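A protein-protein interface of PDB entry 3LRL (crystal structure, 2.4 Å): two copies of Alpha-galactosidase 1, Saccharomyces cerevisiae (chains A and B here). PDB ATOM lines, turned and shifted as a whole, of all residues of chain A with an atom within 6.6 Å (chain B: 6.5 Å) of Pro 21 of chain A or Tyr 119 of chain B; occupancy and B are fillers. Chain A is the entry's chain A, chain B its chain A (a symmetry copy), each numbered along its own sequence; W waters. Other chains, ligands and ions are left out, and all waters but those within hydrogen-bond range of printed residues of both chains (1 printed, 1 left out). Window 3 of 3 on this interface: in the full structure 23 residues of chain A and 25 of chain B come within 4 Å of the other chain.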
ATOM      1  N   VAL A  19      28.093 -30.333  12.525  1.00  0.00           N
ATOM      2  CA  VAL A  19      28.399 -28.866  12.539  1.00  0.00           C
ATOM      3  C   VAL A  19      27.780 -28.210  11.326  1.00  0.00           C
ATOM      4  O   VAL A  19      27.572 -28.855  10.285  1.00  0.00           O
ATOM      5  CB  VAL A  19      29.918 -28.568  12.530  1.00  0.00           C
ATOM      6  CG1 VAL A  19      30.393 -28.127  13.913  1.00  0.00           C
ATOM      7  CG2 VAL A  19      30.705 -29.777  12.040  1.00  0.00           C
ATOM      8  N   SER A  20      27.461 -26.933  11.473  1.00  0.00           N
ATOM      9  CA  SER A  20      26.865 -26.154  10.416  1.00  0.00           C
ATOM     10  C   SER A  20      27.191 -24.722  10.755  1.00  0.00           C
ATOM     11  O   SER A  20      27.359 -24.393  11.938  1.00  0.00           O
ATOM     12  CB  SER A  20      25.331 -26.387  10.329  1.00  0.00           C
ATOM     13  OG  SER A  20      24.634 -26.066  11.538  1.00  0.00           O
ATOM     14  N   PRO A  21      27.300 -23.862   9.727  1.00  0.00           N
ATOM     15  CA  PRO A  21      27.460 -22.441   9.987  1.00  0.00           C
ATOM     16  C   PRO A  21      26.261 -21.897  10.752  1.00  0.00           C
ATOM     17  O   PRO A  21      25.187 -22.469  10.679  1.00  0.00           O
ATOM     18  CB  PRO A  21      27.502 -21.826   8.573  1.00  0.00           C
ATOM     19  CG  PRO A  21      26.868 -22.823   7.707  1.00  0.00           C
ATOM     20  CD  PRO A  21      27.294 -24.146   8.284  1.00  0.00           C
ATOM     21  N   SER A  22      26.443 -20.802  11.477  1.00  0.00           N
ATOM     22  CA  SER A  22      25.305 -20.078  12.026  1.00  0.00           C
ATOM     23  C   SER A  22      24.393 -19.677  10.874  1.00  0.00           C
ATOM     24  O   SER A  22      24.882 -19.305   9.796  1.00  0.00           O
ATOM     25  CB  SER A  22      25.769 -18.841  12.768  1.00  0.00           C
ATOM     26  OG  SER A  22      24.657 -18.108  13.214  1.00  0.00           O
ATOM     27  N   TYR A  23      23.079 -19.732  11.090  1.00  0.00           N
ATOM     28  CA  TYR A  23      22.127 -19.503  10.008  1.00  0.00           C
ATOM     29  C   TYR A  23      22.077 -18.022   9.596  1.00  0.00           C
ATOM     30  O   TYR A  23      21.810 -17.695   8.434  1.00  0.00           O
ATOM     31  CB  TYR A  23      20.737 -20.074  10.375  1.00  0.00           C
ATOM     32  CG  TYR A  23      19.785 -19.081  11.030  1.00  0.00           C
ATOM     33  CD1 TYR A  23      18.758 -18.465  10.286  1.00  0.00           C
ATOM     34  CD2 TYR A  23      19.923 -18.734  12.375  1.00  0.00           C
ATOM     35  CE1 TYR A  23      17.893 -17.538  10.880  1.00  0.00           C
ATOM     36  CE2 TYR A  23      19.069 -17.811  12.969  1.00  0.00           C
ATOM     37  CZ  TYR A  23      18.057 -17.226  12.223  1.00  0.00           C
ATOM     38  OH  TYR A  23      17.224 -16.314  12.818  1.00  0.00           O
ATOM     39  N   ASN A  24      22.338 -17.140  10.558  1.00  0.00           N
ATOM     40  CA  ASN A  24      22.258 -15.695  10.367  1.00  0.00           C
ATOM     41  C   ASN A  24      23.529 -14.927  10.769  1.00  0.00           C
ATOM     42  O   ASN A  24      23.545 -13.678  10.741  1.00  0.00           O
ATOM     43  CB  ASN A  24      21.059 -15.132  11.135  1.00  0.00           C
ATOM     44  CG  ASN A  24      21.169 -15.339  12.631  1.00  0.00           C
ATOM     45  OD1 ASN A  24      22.073 -16.018  13.113  1.00  0.00           O
ATOM     46  ND2 ASN A  24      20.237 -14.749  13.381  1.00  0.00           N
ATOM     47  N   GLY A  25      24.566 -15.668  11.170  1.00  0.00           N
ATOM     48  CA  GLY A  25      25.830 -15.071  11.629  1.00  0.00           C
ATOM     49  C   GLY A  25      25.920 -14.723  13.120  1.00  0.00           C
ATOM     50  O   GLY A  25      26.974 -14.272  13.598  1.00  0.00           O
ATOM     51  N   SER A 198      18.459 -25.172  14.514  1.00  0.00           N
ATOM     52  CA  SER A 198      19.676 -24.468  14.054  1.00  0.00           C
ATOM     53  C   SER A 198      19.564 -23.741  12.716  1.00  0.00           C
ATOM     54  O   SER A 198      20.227 -22.721  12.500  1.00  0.00           O
ATOM     55  CB  SER A 198      20.855 -25.440  14.000  1.00  0.00           C
ATOM     56  OG  SER A 198      20.596 -26.440  13.045  1.00  0.00           O
ATOM     57  N   GLY A 199      18.755 -24.270  11.811  1.00  0.00           N
ATOM     58  CA  GLY A 199      18.687 -23.725  10.460  1.00  0.00           C
ATOM     59  C   GLY A 199      17.784 -22.519  10.366  1.00  0.00           C
ATOM     60  O   GLY A 199      17.766 -21.814   9.356  1.00  0.00           O
ATOM     61  N   VAL A 255      28.070 -23.858  17.586  1.00  0.00           N
ATOM     62  CA  VAL A 255      28.195 -22.486  17.059  1.00  0.00           C
ATOM     63  C   VAL A 255      26.979 -22.140  16.190  1.00  0.00           C
ATOM     64  O   VAL A 255      26.691 -22.838  15.196  1.00  0.00           O
ATOM     65  CB  VAL A 255      29.498 -22.309  16.201  1.00  0.00           C
ATOM     66  CG1 VAL A 255      29.425 -21.013  15.357  1.00  0.00           C
ATOM     67  CG2 VAL A 255      30.735 -22.326  17.079  1.00  0.00           C
ATOM     68  N   GLY A 256      26.268 -21.085  16.596  1.00  0.00           N
ATOM     69  CA  GLY A 256      25.103 -20.613  15.873  1.00  0.00           C
ATOM     70  C   GLY A 256      23.730 -21.051  16.363  1.00  0.00           C
ATOM     71  O   GLY A 256      22.726 -20.484  15.928  1.00  0.00           O
ATOM     72  N   TYR B 113      29.462 -39.976  -0.417  1.00  0.00           N
ATOM     73  CA  TYR B 113      28.611 -39.617   0.693  1.00  0.00           C
ATOM     74  C   TYR B 113      27.976 -38.232   0.469  1.00  0.00           C
ATOM     75  O   TYR B 113      28.606 -37.291  -0.078  1.00  0.00           O
ATOM     76  CB  TYR B 113      29.444 -39.654   1.992  1.00  0.00           C
ATOM     77  CG  TYR B 113      28.837 -38.926   3.153  1.00  0.00           C
ATOM     78  CD1 TYR B 113      28.936 -37.530   3.261  1.00  0.00           C
ATOM     79  CD2 TYR B 113      28.151 -39.618   4.142  1.00  0.00           C
ATOM     80  CE1 TYR B 113      28.362 -36.850   4.309  1.00  0.00           C
ATOM     81  CE2 TYR B 113      27.576 -38.947   5.202  1.00  0.00           C
ATOM     82  CZ  TYR B 113      27.688 -37.569   5.280  1.00  0.00           C
ATOM     83  OH  TYR B 113      27.100 -36.913   6.328  1.00  0.00           O
ATOM     84  N   SER B 114      26.719 -38.120   0.906  1.00  0.00           N
ATOM     85  CA  SER B 114      26.057 -36.820   1.122  1.00  0.00           C
ATOM     86  C   SER B 114      25.054 -36.956   2.284  1.00  0.00           C
ATOM     87  O   SER B 114      25.000 -37.996   2.947  1.00  0.00           O
ATOM     88  CB  SER B 114      25.342 -36.345  -0.144  1.00  0.00           C
ATOM     89  OG  SER B 114      25.098 -34.945  -0.061  1.00  0.00           O
ATOM     90  N   SER B 115      24.257 -35.913   2.507  1.00  0.00           N
ATOM     91  CA  SER B 115      23.209 -35.939   3.516  1.00  0.00           C
ATOM     92  C   SER B 115      21.891 -35.408   2.945  1.00  0.00           C
ATOM     93  O   SER B 115      21.875 -34.401   2.212  1.00  0.00           O
ATOM     94  CB  SER B 115      23.661 -35.122   4.747  1.00  0.00           C
ATOM     95  OG  SER B 115      22.683 -35.094   5.767  1.00  0.00           O
ATOM     96  N   ALA B 116      20.792 -36.097   3.268  1.00  0.00           N
ATOM     97  CA  ALA B 116      19.428 -35.605   2.997  1.00  0.00           C
ATOM     98  C   ALA B 116      19.097 -34.439   3.931  1.00  0.00           C
ATOM     99  O   ALA B 116      18.211 -34.508   4.784  1.00  0.00           O
ATOM    100  CB  ALA B 116      18.422 -36.702   3.156  1.00  0.00           C
ATOM    101  N   GLY B 117      19.829 -33.357   3.751  1.00  0.00           N
ATOM    102  CA  GLY B 117      19.614 -32.149   4.491  1.00  0.00           C
ATOM    103  C   GLY B 117      20.393 -31.030   3.849  1.00  0.00           C
ATOM    104  O   GLY B 117      21.038 -31.203   2.818  1.00  0.00           O
ATOM    105  N   GLU B 118      20.321 -29.873   4.489  1.00  0.00           N
ATOM    106  CA  GLU B 118      20.999 -28.673   4.045  1.00  0.00           C
ATOM    107  C   GLU B 118      22.530 -28.783   4.120  1.00  0.00           C
ATOM    108  O   GLU B 118      23.267 -28.242   3.287  1.00  0.00           O
ATOM    109  CB  GLU B 118      20.517 -27.541   4.922  1.00  0.00           C
ATOM    110  CG  GLU B 118      20.881 -26.203   4.417  1.00  0.00           C
ATOM    111  CD  GLU B 118      20.492 -25.104   5.375  1.00  0.00           C
ATOM    112  OE1 GLU B 118      20.801 -23.937   5.024  1.00  0.00           O
ATOM    113  OE2 GLU B 118      19.892 -25.390   6.466  1.00  0.00           O
ATOM    114  N   TYR B 119      23.012 -29.472   5.132  1.00  0.00           N
ATOM    115  CA  TYR B 119      24.448 -29.669   5.274  1.00  0.00           C
ATOM    116  C   TYR B 119      24.668 -31.146   5.534  1.00  0.00           C
ATOM    117  O   TYR B 119      23.722 -31.868   5.905  1.00  0.00           O
ATOM    118  CB  TYR B 119      25.020 -28.812   6.431  1.00  0.00           C
ATOM    119  CG  TYR B 119      24.779 -27.325   6.265  1.00  0.00           C
ATOM    120  CD1 TYR B 119      23.742 -26.690   6.938  1.00  0.00           C
ATOM    121  CD2 TYR B 119      25.575 -26.561   5.410  1.00  0.00           C
ATOM    122  CE1 TYR B 119      23.501 -25.321   6.775  1.00  0.00           C
ATOM    123  CE2 TYR B 119      25.352 -25.185   5.227  1.00  0.00           C
ATOM    124  CZ  TYR B 119      24.312 -24.569   5.915  1.00  0.00           C
ATOM    125  OH  TYR B 119      24.087 -23.210   5.744  1.00  0.00           O
ATOM    126  N   THR B 120      25.902 -31.597   5.334  1.00  0.00           N
ATOM    127  CA  THR B 120      26.307 -32.905   5.821  1.00  0.00           C
ATOM    128  C   THR B 120      26.532 -32.804   7.337  1.00  0.00           C
ATOM    129  O   THR B 120      26.527 -31.701   7.906  1.00  0.00           O
ATOM    130  CB  THR B 120      27.577 -33.420   5.088  1.00  0.00           C
ATOM    131  OG1 THR B 120      28.696 -32.590   5.410  1.00  0.00           O
ATOM    132  CG2 THR B 120      27.378 -33.440   3.564  1.00  0.00           C
ATOM    133  N   CYS B 121      26.725 -33.928   8.012  1.00  0.00           N
ATOM    134  CA  CYS B 121      26.935 -33.869   9.474  1.00  0.00           C
ATOM    135  C   CYS B 121      28.131 -33.030   9.891  1.00  0.00           C
ATOM    136  O   CYS B 121      28.085 -32.389  10.927  1.00  0.00           O
ATOM    137  CB  CYS B 121      27.006 -35.251  10.102  1.00  0.00           C
ATOM    138  SG  CYS B 121      25.554 -36.240   9.773  1.00  0.00           S
ATOM    139  N   ALA B 122      29.185 -33.005   9.078  1.00  0.00           N
ATOM    140  CA  ALA B 122      30.371 -32.174   9.358  1.00  0.00           C
ATOM    141  C   ALA B 122      30.278 -30.764   8.755  1.00  0.00           C
ATOM    142  O   ALA B 122      31.251 -30.005   8.779  1.00  0.00           O
ATOM    143  CB  ALA B 122      31.632 -32.870   8.895  1.00  0.00           C
ATOM    144  N   GLY B 123      29.114 -30.425   8.198  1.00  0.00           N
ATOM    145  CA  GLY B 123      28.828 -29.046   7.773  1.00  0.00           C
ATOM    146  C   GLY B 123      29.140 -28.693   6.333  1.00  0.00           C
ATOM    147  O   GLY B 123      29.123 -27.509   5.951  1.00  0.00           O
ATOM    148  N   TYR B 124      29.399 -29.706   5.524  1.00  0.00           N
ATOM    149  CA  TYR B 124      29.618 -29.492   4.091  1.00  0.00           C
ATOM    150  C   TYR B 124      28.274 -29.403   3.355  1.00  0.00           C
ATOM    151  O   TYR B 124      27.241 -29.641   3.953  1.00  0.00           O
ATOM    152  CB  TYR B 124      30.570 -30.561   3.523  1.00  0.00           C
ATOM    153  CG  TYR B 124      31.969 -30.424   4.098  1.00  0.00           C
ATOM    154  CD1 TYR B 124      32.259 -30.864   5.393  1.00  0.00           C
ATOM    155  CD2 TYR B 124      32.979 -29.802   3.375  1.00  0.00           C
ATOM    156  CE1 TYR B 124      33.531 -30.701   5.951  1.00  0.00           C
ATOM    157  CE2 TYR B 124      34.260 -29.650   3.906  1.00  0.00           C
ATOM    158  CZ  TYR B 124      34.529 -30.093   5.199  1.00  0.00           C
ATOM    159  OH  TYR B 124      35.795 -29.949   5.726  1.00  0.00           O
ATOM    160  N   PRO B 125      28.283 -29.004   2.067  1.00  0.00           N
ATOM    161  CA  PRO B 125      27.038 -28.922   1.284  1.00  0.00           C
ATOM    162  C   PRO B 125      26.238 -30.234   1.308  1.00  0.00           C
ATOM    163  O   PRO B 125      26.799 -31.277   0.986  1.00  0.00           O
ATOM    164  CB  PRO B 125      27.549 -28.683  -0.139  1.00  0.00           C
ATOM    165  CG  PRO B 125      28.851 -28.055   0.026  1.00  0.00           C
ATOM    166  CD  PRO B 125      29.461 -28.599   1.266  1.00  0.00           C
ATOM    167  N   GLY B 126      24.947 -30.162   1.663  1.00  0.00           N
ATOM    168  CA  GLY B 126      24.042 -31.314   1.634  1.00  0.00           C
ATOM    169  C   GLY B 126      23.186 -31.345   0.365  1.00  0.00           C
ATOM    170  O   GLY B 126      23.187 -30.390  -0.403  1.00  0.00           O
ATOM    171  N   SER B 127      22.428 -32.418   0.154  1.00  0.00           N
ATOM    172  CA  SER B 127      21.738 -32.601  -1.120  1.00  0.00           C
ATOM    173  C   SER B 127      20.243 -32.332  -1.116  1.00  0.00           C
ATOM    174  O   SER B 127      19.624 -32.432  -2.163  1.00  0.00           O
ATOM    175  CB  SER B 127      21.973 -34.009  -1.664  1.00  0.00           C
ATOM    176  OG  SER B 127      23.336 -34.240  -1.954  1.00  0.00           O
ATOM    177  N   ASN B 150      21.455 -38.028   7.336  1.00  0.00           N
ATOM    178  CA  ASN B 150      20.199 -37.431   7.828  1.00  0.00           C
ATOM    179  C   ASN B 150      20.370 -36.188   8.717  1.00  0.00           C
ATOM    180  O   ASN B 150      19.474 -35.816   9.488  1.00  0.00           O
ATOM    181  CB  ASN B 150      19.392 -38.502   8.552  1.00  0.00           C
ATOM    182  CG  ASN B 150      17.986 -38.035   8.979  1.00  0.00           C
ATOM    183  OD1 ASN B 150      17.288 -37.326   8.260  1.00  0.00           O
ATOM    184  ND2 ASN B 150      17.573 -38.468  10.146  1.00  0.00           N
ATOM    185  N   CYS B 151      21.528 -35.554   8.613  1.00  0.00           N
ATOM    186  CA  CYS B 151      21.806 -34.319   9.342  1.00  0.00           C
ATOM    187  C   CYS B 151      21.171 -33.115   8.642  1.00  0.00           C
ATOM    188  O   CYS B 151      21.102 -33.069   7.413  1.00  0.00           O
ATOM    189  CB  CYS B 151      23.322 -34.129   9.522  1.00  0.00           C
ATOM    190  SG  CYS B 151      24.048 -35.275  10.766  1.00  0.00           S
ATOM    191  N   TYR B 152      20.698 -32.166   9.449  1.00  0.00           N
ATOM    192  CA  TYR B 152      20.135 -30.891   8.996  1.00  0.00           C
ATOM    193  C   TYR B 152      19.037 -31.095   7.947  1.00  0.00           C
ATOM    194  O   TYR B 152      19.051 -30.499   6.874  1.00  0.00           O
ATOM    195  CB  TYR B 152      21.262 -29.924   8.533  1.00  0.00           C
ATOM    196  CG  TYR B 152      22.332 -29.765   9.592  1.00  0.00           C
ATOM    197  CD1 TYR B 152      23.575 -30.399   9.465  1.00  0.00           C
ATOM    198  CD2 TYR B 152      22.088 -29.008  10.745  1.00  0.00           C
ATOM    199  CE1 TYR B 152      24.557 -30.280  10.463  1.00  0.00           C
ATOM    200  CE2 TYR B 152      23.044 -28.883  11.743  1.00  0.00           C
ATOM    201  CZ  TYR B 152      24.273 -29.520  11.601  1.00  0.00           C
ATOM    202  OH  TYR B 152      25.209 -29.392  12.609  1.00  0.00           O
ATOM    203  N   ASN B 153      18.071 -31.938   8.285  1.00  0.00           N
ATOM    204  CA  ASN B 153      17.023 -32.313   7.337  1.00  0.00           C
ATOM    205  C   ASN B 153      15.863 -31.326   7.248  1.00  0.00           C
ATOM    206  O   ASN B 153      14.876 -31.583   6.567  1.00  0.00           O
ATOM    207  CB  ASN B 153      16.529 -33.730   7.622  1.00  0.00           C
ATOM    208  CG  ASN B 153      16.046 -33.904   9.049  1.00  0.00           C
ATOM    209  OD1 ASN B 153      15.526 -32.965   9.660  1.00  0.00           O
ATOM    210  ND2 ASN B 153      16.202 -35.113   9.583  1.00  0.00           N
HETATM  211  O   HOH W   1      19.221 -22.734   7.064  1.00  0.00           O
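No position is printed for both chains. Of the 9 pairs that touch across the chains among the printed residues, none has its exchanged pair printed and touching as well.
The backbone NH of Val 19 of chain A lies within hydrogen-bond range of the backbone carbonyl oxygen of Cys 121 of chain B. The backbone carbonyl oxygen (O) of Val 19 of chain A sits close to the backbone NH (N) of Gly 123 of chain B, at 3.0 Å. N of Val 19 of chain A is in hydrogen-bond range of OH of Tyr 152 of chain B.
Of the printed residues of chain B, Val 19 of chain A touches Thr 120, Cys 121, Ala 122, Gly 123 and Tyr 152. Pro 21 of chain A touches one residue of chain B. Of the printed residues of chain A, Tyr 119 of chain B touches Ser 20 (3.8 Å) and Pro 21 (3.4 Å). Printed residues of chain A within 4 Å of Thr 120 of chain B: Val 19. Of the printed residues of chain A, Cys 121 of chain B touches Val 19 (2.6 Å). Printed residues of chain A within 4 Å of Gly 123 of chain B: Val 19. Asn 153 of chain B touches none of the printed residues of chain A. The nearest residue of chain A that does not touch Tyr 119 of chain B is Val 19 of chain A (4.6 Å).
The backbone NH of Cys 121 of chain B lies within hydrogen-bond range of the side-chain hydroxyl of Tyr 113 of chain B (3.4 Å). The side-chain hydroxyl (OG) of Ser 115 of chain B lies within hydrogen-bond range of the backbone carbonyl oxygen (O) of Tyr 119 of chain B (3.4 Å). OE1 of Glu 118 of chain B sits at hydrogen-bond distance from OH of Tyr 119 of chain B (3.4 Å). The backbone NH (N) of Glu 118 of chain B sits at hydrogen-bond distance from the backbone carbonyl oxygen (O) of Tyr 152 of chain B, at 2.8 Å. The backbone NH of Tyr 124 of chain B is in hydrogen-bond range of the side-chain hydroxyl of Thr 120 of chain B (3.0 Å). The side-chain sulfur of Cys 121 of chain B forms a disulfide with the side-chain sulfur of Cys 151 of chain B (2.0 Å).
O of Val 19 of chain A touches O of Thr 120 of chain B, at 3.9 Å. CG2 of Val 19 of chain A touches O of Ala 122 of chain B, at 3.3 Å. Ser 20 of chain A touches Tyr 119 of chain B. Ser 20 of chain A touches Tyr 152 of chain B (OG to CE2, 3.2 Å). Pro 21 of chain A touches Tyr 119 of chain B. Ser 198 of chain A touches Tyr 152 of chain B.
Water W1 bridges OE2 of Glu 118 of chain B and O of Gly 199 of chain A.
Of the 19 printed residues of chain B, 6 touch a printed residue of chain A. Of the 11 printed residues of chain A, 4 touch a printed residue of chain B. Printed residues of chain A that touch a printed residue of chain B: Val 19, Ser 20, Pro 21 and Ser 198. Among the printed residues, no Asp or Glu carboxylate lies within 4 Å of a Lys or Arg side-chain nitrogen of the other chain.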
